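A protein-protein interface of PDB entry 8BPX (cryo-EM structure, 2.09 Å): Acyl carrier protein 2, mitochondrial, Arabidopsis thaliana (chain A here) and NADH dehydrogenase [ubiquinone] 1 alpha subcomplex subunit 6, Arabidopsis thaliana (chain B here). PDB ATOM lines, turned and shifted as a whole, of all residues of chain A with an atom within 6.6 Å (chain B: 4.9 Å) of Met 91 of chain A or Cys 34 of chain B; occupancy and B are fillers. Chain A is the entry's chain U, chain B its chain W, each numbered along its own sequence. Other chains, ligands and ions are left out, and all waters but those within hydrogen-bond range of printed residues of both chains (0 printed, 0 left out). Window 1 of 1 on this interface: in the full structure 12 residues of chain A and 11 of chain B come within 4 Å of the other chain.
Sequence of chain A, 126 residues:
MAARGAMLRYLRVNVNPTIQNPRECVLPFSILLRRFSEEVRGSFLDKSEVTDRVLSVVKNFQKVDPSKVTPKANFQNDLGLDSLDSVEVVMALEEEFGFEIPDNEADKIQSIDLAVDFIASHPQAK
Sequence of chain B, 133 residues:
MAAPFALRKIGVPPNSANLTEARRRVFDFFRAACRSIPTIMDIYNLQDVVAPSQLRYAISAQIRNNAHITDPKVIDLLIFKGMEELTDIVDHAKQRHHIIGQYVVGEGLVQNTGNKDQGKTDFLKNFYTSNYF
Val 87 of chain A touches Phe 30 of chain B.
Phe 30 of chain B touches Glu 88 of chain A.
Met 91 of chain A touches Arg 31 of chain B.
Met 91 of chain A touches Cys 34 of chain B.
Met 91 of chain A touches Arg 35 of chain B (CE to CG, 3.7 Å).
The side-chain carboxylate (OE2) of Glu 94 of chain A lies within salt-bridge range of the guanidinium group (NH2) of Arg 35 of chain B (3.3 Å).
The side-chain carboxylate of Glu 95 of chain A lies within salt-bridge range of the guanidinium group of Arg 56 of chain B.
The backbone carbonyl oxygen (O) of Ile 101 of chain A sits at hydrogen-bond distance from the guanidinium group (NH2) of Arg 35 of chain B (3.3 Å).
Ser 86 of chain A touches none of the printed residues of chain B.
Of the printed residues of chain B, Val 87 of chain A touches Phe 30 (3.7 Å).
Of chain B, only Arg 31 (3.9 Å), Cys 34 (3.4 Å) and Arg 35 (3.7 Å) come within 4 Å of Met 91 of chain A.
Leu 93 of chain A touches none of the printed residues of chain B.
Printed residues of chain B within 4 Å of Glu 95 of chain A: Arg 56.
Printed residues of chain A within 4 Å of Phe 30 of chain B: Val 87 (3.7 Å) and Glu 88 (3.8 Å).
Of the printed residues of chain A, Arg 31 of chain B touches Met 91 (3.9 Å).
Printed residues of chain B that touch a printed residue of chain A: Phe 30, Arg 31, Cys 34, Arg 35 and Arg 56.
Along chain B the printed residues that touch a printed residue of chain A span positions 30 to 56.
Hydrophobic or aromatic side chains of chain A that line the printed part of chain B: Val 87 and Met 91.
Among the printed residues, 8 pairs touch across the chains.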
ATOM      1  N   SER A  86     -23.268   4.936 -12.003  1.00  0.00           N
ATOM      2  CA  SER A  86     -24.137   4.497 -13.092  1.00  0.00           C
ATOM      3  C   SER A  86     -24.384   2.993 -13.030  1.00  0.00           C
ATOM      4  O   SER A  86     -25.510   2.529 -13.256  1.00  0.00           O
ATOM      5  CB  SER A  86     -23.541   4.894 -14.444  1.00  0.00           C
ATOM      6  OG  SER A  86     -22.424   4.092 -14.774  1.00  0.00           O
ATOM      7  N   VAL A  87     -23.344   2.216 -12.719  1.00  0.00           N
ATOM      8  CA  VAL A  87     -23.527   0.782 -12.495  1.00  0.00           C
ATOM      9  C   VAL A  87     -24.471   0.552 -11.323  1.00  0.00           C
ATOM     10  O   VAL A  87     -25.319  -0.349 -11.354  1.00  0.00           O
ATOM     11  CB  VAL A  87     -22.163   0.103 -12.266  1.00  0.00           C
ATOM     12  CG1 VAL A  87     -22.322  -1.158 -11.435  1.00  0.00           C
ATOM     13  CG2 VAL A  87     -21.495  -0.210 -13.582  1.00  0.00           C
ATOM     14  N   GLU A  88     -24.331   1.357 -10.268  1.00  0.00           N
ATOM     15  CA  GLU A  88     -25.231   1.283  -9.122  1.00  0.00           C
ATOM     16  C   GLU A  88     -26.680   1.472  -9.555  1.00  0.00           C
ATOM     17  O   GLU A  88     -27.568   0.701  -9.175  1.00  0.00           O
ATOM     18  CB  GLU A  88     -24.850   2.369  -8.121  1.00  0.00           C
ATOM     19  CG  GLU A  88     -24.407   1.928  -6.756  1.00  0.00           C
ATOM     20  CD  GLU A  88     -23.829   3.095  -5.980  1.00  0.00           C
ATOM     21  OE1 GLU A  88     -22.725   2.962  -5.431  1.00  0.00           O
ATOM     22  OE2 GLU A  88     -24.488   4.150  -5.906  1.00  0.00           O
ATOM     23  N   VAL A  89     -26.931   2.511 -10.353  1.00  0.00           N
ATOM     24  CA  VAL A  89     -28.287   2.816 -10.800  1.00  0.00           C
ATOM     25  C   VAL A  89     -28.837   1.679 -11.649  1.00  0.00           C
ATOM     26  O   VAL A  89     -30.000   1.279 -11.505  1.00  0.00           O
ATOM     27  CB  VAL A  89     -28.307   4.156 -11.561  1.00  0.00           C
ATOM     28  CG1 VAL A  89     -29.422   4.175 -12.583  1.00  0.00           C
ATOM     29  CG2 VAL A  89     -28.459   5.311 -10.591  1.00  0.00           C
ATOM     30  N   VAL A  90     -28.014   1.137 -12.550  1.00  0.00           N
ATOM     31  CA  VAL A  90     -28.470   0.030 -13.385  1.00  0.00           C
ATOM     32  C   VAL A  90     -28.793  -1.190 -12.529  1.00  0.00           C
ATOM     33  O   VAL A  90     -29.775  -1.900 -12.783  1.00  0.00           O
ATOM     34  CB  VAL A  90     -27.431  -0.294 -14.472  1.00  0.00           C
ATOM     35  CG1 VAL A  90     -27.797  -1.581 -15.185  1.00  0.00           C
ATOM     36  CG2 VAL A  90     -27.339   0.851 -15.462  1.00  0.00           C
ATOM     37  N   MET A  91     -27.987  -1.448 -11.494  1.00  0.00           N
ATOM     38  CA  MET A  91     -28.297  -2.557 -10.597  1.00  0.00           C
ATOM     39  C   MET A  91     -29.592  -2.293  -9.841  1.00  0.00           C
ATOM     40  O   MET A  91     -30.323  -3.232  -9.506  1.00  0.00           O
ATOM     41  CB  MET A  91     -27.161  -2.797  -9.602  1.00  0.00           C
ATOM     42  CG  MET A  91     -25.928  -3.481 -10.191  1.00  0.00           C
ATOM     43  SD  MET A  91     -26.118  -5.225 -10.624  1.00  0.00           S
ATOM     44  CE  MET A  91     -27.046  -5.871  -9.248  1.00  0.00           C
ATOM     45  N   ALA A  92     -29.872  -1.023  -9.540  1.00  0.00           N
ATOM     46  CA  ALA A  92     -31.149  -0.662  -8.933  1.00  0.00           C
ATOM     47  C   ALA A  92     -32.305  -0.941  -9.883  1.00  0.00           C
ATOM     48  O   ALA A  92     -33.382  -1.368  -9.454  1.00  0.00           O
ATOM     49  CB  ALA A  92     -31.140   0.807  -8.515  1.00  0.00           C
ATOM     50  N   LEU A  93     -32.100  -0.699 -11.182  1.00  0.00           N
ATOM     51  CA  LEU A  93     -33.119  -1.038 -12.172  1.00  0.00           C
ATOM     52  C   LEU A  93     -33.460  -2.522 -12.133  1.00  0.00           C
ATOM     53  O   LEU A  93     -34.603  -2.904 -12.405  1.00  0.00           O
ATOM     54  CB  LEU A  93     -32.648  -0.652 -13.578  1.00  0.00           C
ATOM     55  CG  LEU A  93     -32.700   0.815 -14.021  1.00  0.00           C
ATOM     56  CD1 LEU A  93     -32.376   0.932 -15.502  1.00  0.00           C
ATOM     57  CD2 LEU A  93     -34.048   1.438 -13.722  1.00  0.00           C
ATOM     58  N   GLU A  94     -32.481  -3.369 -11.806  1.00  0.00           N
ATOM     59  CA  GLU A  94     -32.710  -4.813 -11.761  1.00  0.00           C
ATOM     60  C   GLU A  94     -33.635  -5.204 -10.617  1.00  0.00           C
ATOM     61  O   GLU A  94     -34.541  -6.024 -10.791  1.00  0.00           O
ATOM     62  CB  GLU A  94     -31.376  -5.544 -11.631  1.00  0.00           C
ATOM     63  CG  GLU A  94     -30.536  -5.498 -12.873  1.00  0.00           C
ATOM     64  CD  GLU A  94     -29.089  -5.865 -12.619  1.00  0.00           C
ATOM     65  OE1 GLU A  94     -28.230  -4.970 -12.750  1.00  0.00           O
ATOM     66  OE2 GLU A  94     -28.813  -7.036 -12.281  1.00  0.00           O
ATOM     67  N   GLU A  95     -33.402  -4.647  -9.427  1.00  0.00           N
ATOM     68  CA  GLU A  95     -34.227  -5.006  -8.281  1.00  0.00           C
ATOM     69  C   GLU A  95     -35.668  -4.557  -8.473  1.00  0.00           C
ATOM     70  O   GLU A  95     -36.604  -5.309  -8.184  1.00  0.00           O
ATOM     71  CB  GLU A  95     -33.646  -4.403  -7.003  1.00  0.00           C
ATOM     72  CG  GLU A  95     -34.591  -4.443  -5.814  1.00  0.00           C
ATOM     73  CD  GLU A  95     -34.218  -3.442  -4.739  1.00  0.00           C
ATOM     74  OE1 GLU A  95     -33.087  -2.916  -4.786  1.00  0.00           O
ATOM     75  OE2 GLU A  95     -35.056  -3.182  -3.850  1.00  0.00           O
ATOM     76  N   GLU A  96     -35.866  -3.339  -8.977  1.00  0.00           N
ATOM     77  CA  GLU A  96     -37.211  -2.795  -9.096  1.00  0.00           C
ATOM     78  C   GLU A  96     -38.059  -3.537 -10.118  1.00  0.00           C
ATOM     79  O   GLU A  96     -39.284  -3.583  -9.967  1.00  0.00           O
ATOM     80  CB  GLU A  96     -37.139  -1.312  -9.442  1.00  0.00           C
ATOM     81  CG  GLU A  96     -36.635  -0.471  -8.285  1.00  0.00           C
ATOM     82  CD  GLU A  96     -37.491  -0.629  -7.042  1.00  0.00           C
ATOM     83  OE1 GLU A  96     -38.715  -0.399  -7.130  1.00  0.00           O
ATOM     84  OE2 GLU A  96     -36.940  -0.981  -5.978  1.00  0.00           O
ATOM     85  N   ILE A 101     -30.180  -7.855 -15.883  1.00  0.00           N
ATOM     86  CA  ILE A 101     -29.860  -7.312 -17.198  1.00  0.00           C
ATOM     87  C   ILE A 101     -28.468  -7.799 -17.585  1.00  0.00           C
ATOM     88  O   ILE A 101     -27.530  -7.695 -16.782  1.00  0.00           O
ATOM     89  CB  ILE A 101     -29.949  -5.779 -17.218  1.00  0.00           C
ATOM     90  CG1 ILE A 101     -29.284  -5.222 -18.470  1.00  0.00           C
ATOM     91  CG2 ILE A 101     -29.256  -5.189 -16.016  1.00  0.00           C
ATOM     92  CD1 ILE A 101     -29.432  -3.732 -18.608  1.00  0.00           C
ATOM     93  N   PHE B  30     -18.520  -6.074  -7.995  1.00  0.00           N
ATOM     94  CA  PHE B  30     -19.618  -5.314  -7.408  1.00  0.00           C
ATOM     95  C   PHE B  30     -20.967  -5.849  -7.869  1.00  0.00           C
ATOM     96  O   PHE B  30     -21.911  -5.950  -7.074  1.00  0.00           O
ATOM     97  CB  PHE B  30     -19.470  -3.835  -7.759  1.00  0.00           C
ATOM     98  CG  PHE B  30     -20.566  -2.968  -7.217  1.00  0.00           C
ATOM     99  CD1 PHE B  30     -20.829  -2.924  -5.859  1.00  0.00           C
ATOM    100  CD2 PHE B  30     -21.335  -2.194  -8.068  1.00  0.00           C
ATOM    101  CE1 PHE B  30     -21.835  -2.122  -5.361  1.00  0.00           C
ATOM    102  CE2 PHE B  30     -22.340  -1.391  -7.573  1.00  0.00           C
ATOM    103  CZ  PHE B  30     -22.591  -1.356  -6.219  1.00  0.00           C
ATOM    104  N   ARG B  31     -21.075  -6.204  -9.151  1.00  0.00           N
ATOM    105  CA  ARG B  31     -22.311  -6.803  -9.644  1.00  0.00           C
ATOM    106  C   ARG B  31     -22.592  -8.132  -8.955  1.00  0.00           C
ATOM    107  O   ARG B  31     -23.725  -8.395  -8.535  1.00  0.00           O
ATOM    108  CB  ARG B  31     -22.237  -6.989 -11.157  1.00  0.00           C
ATOM    109  CG  ARG B  31     -22.450  -5.709 -11.933  1.00  0.00           C
ATOM    110  CD  ARG B  31     -22.569  -5.969 -13.415  1.00  0.00           C
ATOM    111  NE  ARG B  31     -21.911  -4.925 -14.188  1.00  0.00           N
ATOM    112  CZ  ARG B  31     -20.648  -4.976 -14.590  1.00  0.00           C
ATOM    113  NH1 ARG B  31     -19.879  -6.017 -14.321  1.00  0.00           N
ATOM    114  NH2 ARG B  31     -20.147  -3.955 -15.277  1.00  0.00           N
ATOM    115  N   ALA B  32     -21.568  -8.979  -8.818  1.00  0.00           N
ATOM    116  CA  ALA B  32     -21.770 -10.268  -8.161  1.00  0.00           C
ATOM    117  C   ALA B  32     -22.174 -10.090  -6.701  1.00  0.00           C
ATOM    118  O   ALA B  32     -23.020 -10.831  -6.189  1.00  0.00           O
ATOM    119  CB  ALA B  32     -20.507 -11.121  -8.272  1.00  0.00           C
ATOM    120  N   ALA B  33     -21.578  -9.115  -6.014  1.00  0.00           N
ATOM    121  CA  ALA B  33     -21.923  -8.871  -4.617  1.00  0.00           C
ATOM    122  C   ALA B  33     -23.355  -8.366  -4.484  1.00  0.00           C
ATOM    123  O   ALA B  33     -24.098  -8.809  -3.603  1.00  0.00           O
ATOM    124  CB  ALA B  33     -20.945  -7.877  -3.993  1.00  0.00           C
ATOM    125  N   CYS B  34     -23.759  -7.437  -5.351  1.00  0.00           N
ATOM    126  CA  CYS B  34     -25.115  -6.906  -5.261  1.00  0.00           C
ATOM    127  C   CYS B  34     -26.159  -7.962  -5.598  1.00  0.00           C
ATOM    128  O   CYS B  34     -27.206  -8.032  -4.946  1.00  0.00           O
ATOM    129  CB  CYS B  34     -25.279  -5.700  -6.176  1.00  0.00           C
ATOM    130  SG  CYS B  34     -26.915  -4.971  -6.013  1.00  0.00           S
ATOM    131  N   ARG B  35     -25.900  -8.791  -6.611  1.00  0.00           N
ATOM    132  CA  ARG B  35     -26.887  -9.786  -7.010  1.00  0.00           C
ATOM    133  C   ARG B  35     -27.132 -10.831  -5.929  1.00  0.00           C
ATOM    134  O   ARG B  35     -28.170 -11.499  -5.954  1.00  0.00           O
ATOM    135  CB  ARG B  35     -26.449 -10.465  -8.308  1.00  0.00           C
ATOM    136  CG  ARG B  35     -26.567  -9.558  -9.516  1.00  0.00           C
ATOM    137  CD  ARG B  35     -26.172 -10.254 -10.796  1.00  0.00           C
ATOM    138  NE  ARG B  35     -26.530  -9.449 -11.955  1.00  0.00           N
ATOM    139  CZ  ARG B  35     -25.655  -8.937 -12.809  1.00  0.00           C
ATOM    140  NH1 ARG B  35     -24.356  -9.152 -12.678  1.00  0.00           N
ATOM    141  NH2 ARG B  35     -26.092  -8.181 -13.811  1.00  0.00           N
ATOM    142  N   SER B  36     -26.213 -10.980  -4.981  1.00  0.00           N
ATOM    143  CA  SER B  36     -26.364 -11.936  -3.893  1.00  0.00           C
ATOM    144  C   SER B  36     -27.084 -11.352  -2.682  1.00  0.00           C
ATOM    145  O   SER B  36     -27.193 -12.033  -1.658  1.00  0.00           O
ATOM    146  CB  SER B  36     -24.990 -12.466  -3.473  1.00  0.00           C
ATOM    147  OG  SER B  36     -24.477 -11.730  -2.383  1.00  0.00           O
ATOM    148  N   ILE B  37     -27.559 -10.109  -2.769  1.00  0.00           N
ATOM    149  CA  ILE B  37     -28.219  -9.485  -1.621  1.00  0.00           C
ATOM    150  C   ILE B  37     -29.503 -10.204  -1.213  1.00  0.00           C
ATOM    151  O   ILE B  37     -29.709 -10.408  -0.007  1.00  0.00           O
ATOM    152  CB  ILE B  37     -28.436  -7.983  -1.889  1.00  0.00           C
ATOM    153  CG1 ILE B  37     -27.127  -7.221  -1.689  1.00  0.00           C
ATOM    154  CG2 ILE B  37     -29.499  -7.414  -0.968  1.00  0.00           C
ATOM    155  CD1 ILE B  37     -27.145  -5.833  -2.265  1.00  0.00           C
ATOM    156  N   PRO B  38     -30.411 -10.577  -2.130  1.00  0.00           N
ATOM    157  CA  PRO B  38     -31.624 -11.293  -1.683  1.00  0.00           C
ATOM    158  C   PRO B  38     -31.339 -12.602  -0.960  1.00  0.00           C
ATOM    159  O   PRO B  38     -32.022 -12.928   0.023  1.00  0.00           O
ATOM    160  CB  PRO B  38     -32.391 -11.522  -2.992  1.00  0.00           C
ATOM    161  CG  PRO B  38     -31.931 -10.437  -3.886  1.00  0.00           C
ATOM    162  CD  PRO B  38     -30.480 -10.255  -3.568  1.00  0.00           C
ATOM    163  N   ARG B  56     -26.399  -2.695  -0.488  1.00  0.00           N
ATOM    164  CA  ARG B  56     -25.759  -2.161  -1.685  1.00  0.00           C
ATOM    165  C   ARG B  56     -24.916  -0.940  -1.361  1.00  0.00           C
ATOM    166  O   ARG B  56     -23.785  -0.803  -1.847  1.00  0.00           O
ATOM    167  CB  ARG B  56     -26.820  -1.810  -2.727  1.00  0.00           C
ATOM    168  CG  ARG B  56     -26.454  -2.194  -4.130  1.00  0.00           C
ATOM    169  CD  ARG B  56     -27.488  -1.721  -5.145  1.00  0.00           C
ATOM    170  NE  ARG B  56     -27.937  -0.353  -4.927  1.00  0.00           N
ATOM    171  CZ  ARG B  56     -29.206  -0.010  -4.756  1.00  0.00           C
ATOM    172  NH1 ARG B  56     -30.175  -0.909  -4.788  1.00  0.00           N
ATOM    173  NH2 ARG B  56     -29.509   1.269  -4.551  1.00  0.00           N
ATOM    174  N   ILE B  59     -21.674  -1.937   0.392  1.00  0.00           N
ATOM    175  CA  ILE B  59     -20.700  -2.502  -0.540  1.00  0.00           C
ATOM    176  C   ILE B  59     -20.043  -1.394  -1.357  1.00  0.00           C
ATOM    177  O   ILE B  59     -18.812  -1.346  -1.513  1.00  0.00           O
ATOM    178  CB  ILE B  59     -21.363  -3.550  -1.451  1.00  0.00           C
ATOM    179  CG1 ILE B  59     -21.923  -4.706  -0.631  1.00  0.00           C
ATOM    180  CG2 ILE B  59     -20.364  -4.085  -2.459  1.00  0.00           C
ATOM    181  CD1 ILE B  59     -22.740  -5.672  -1.454  1.00  0.00           C
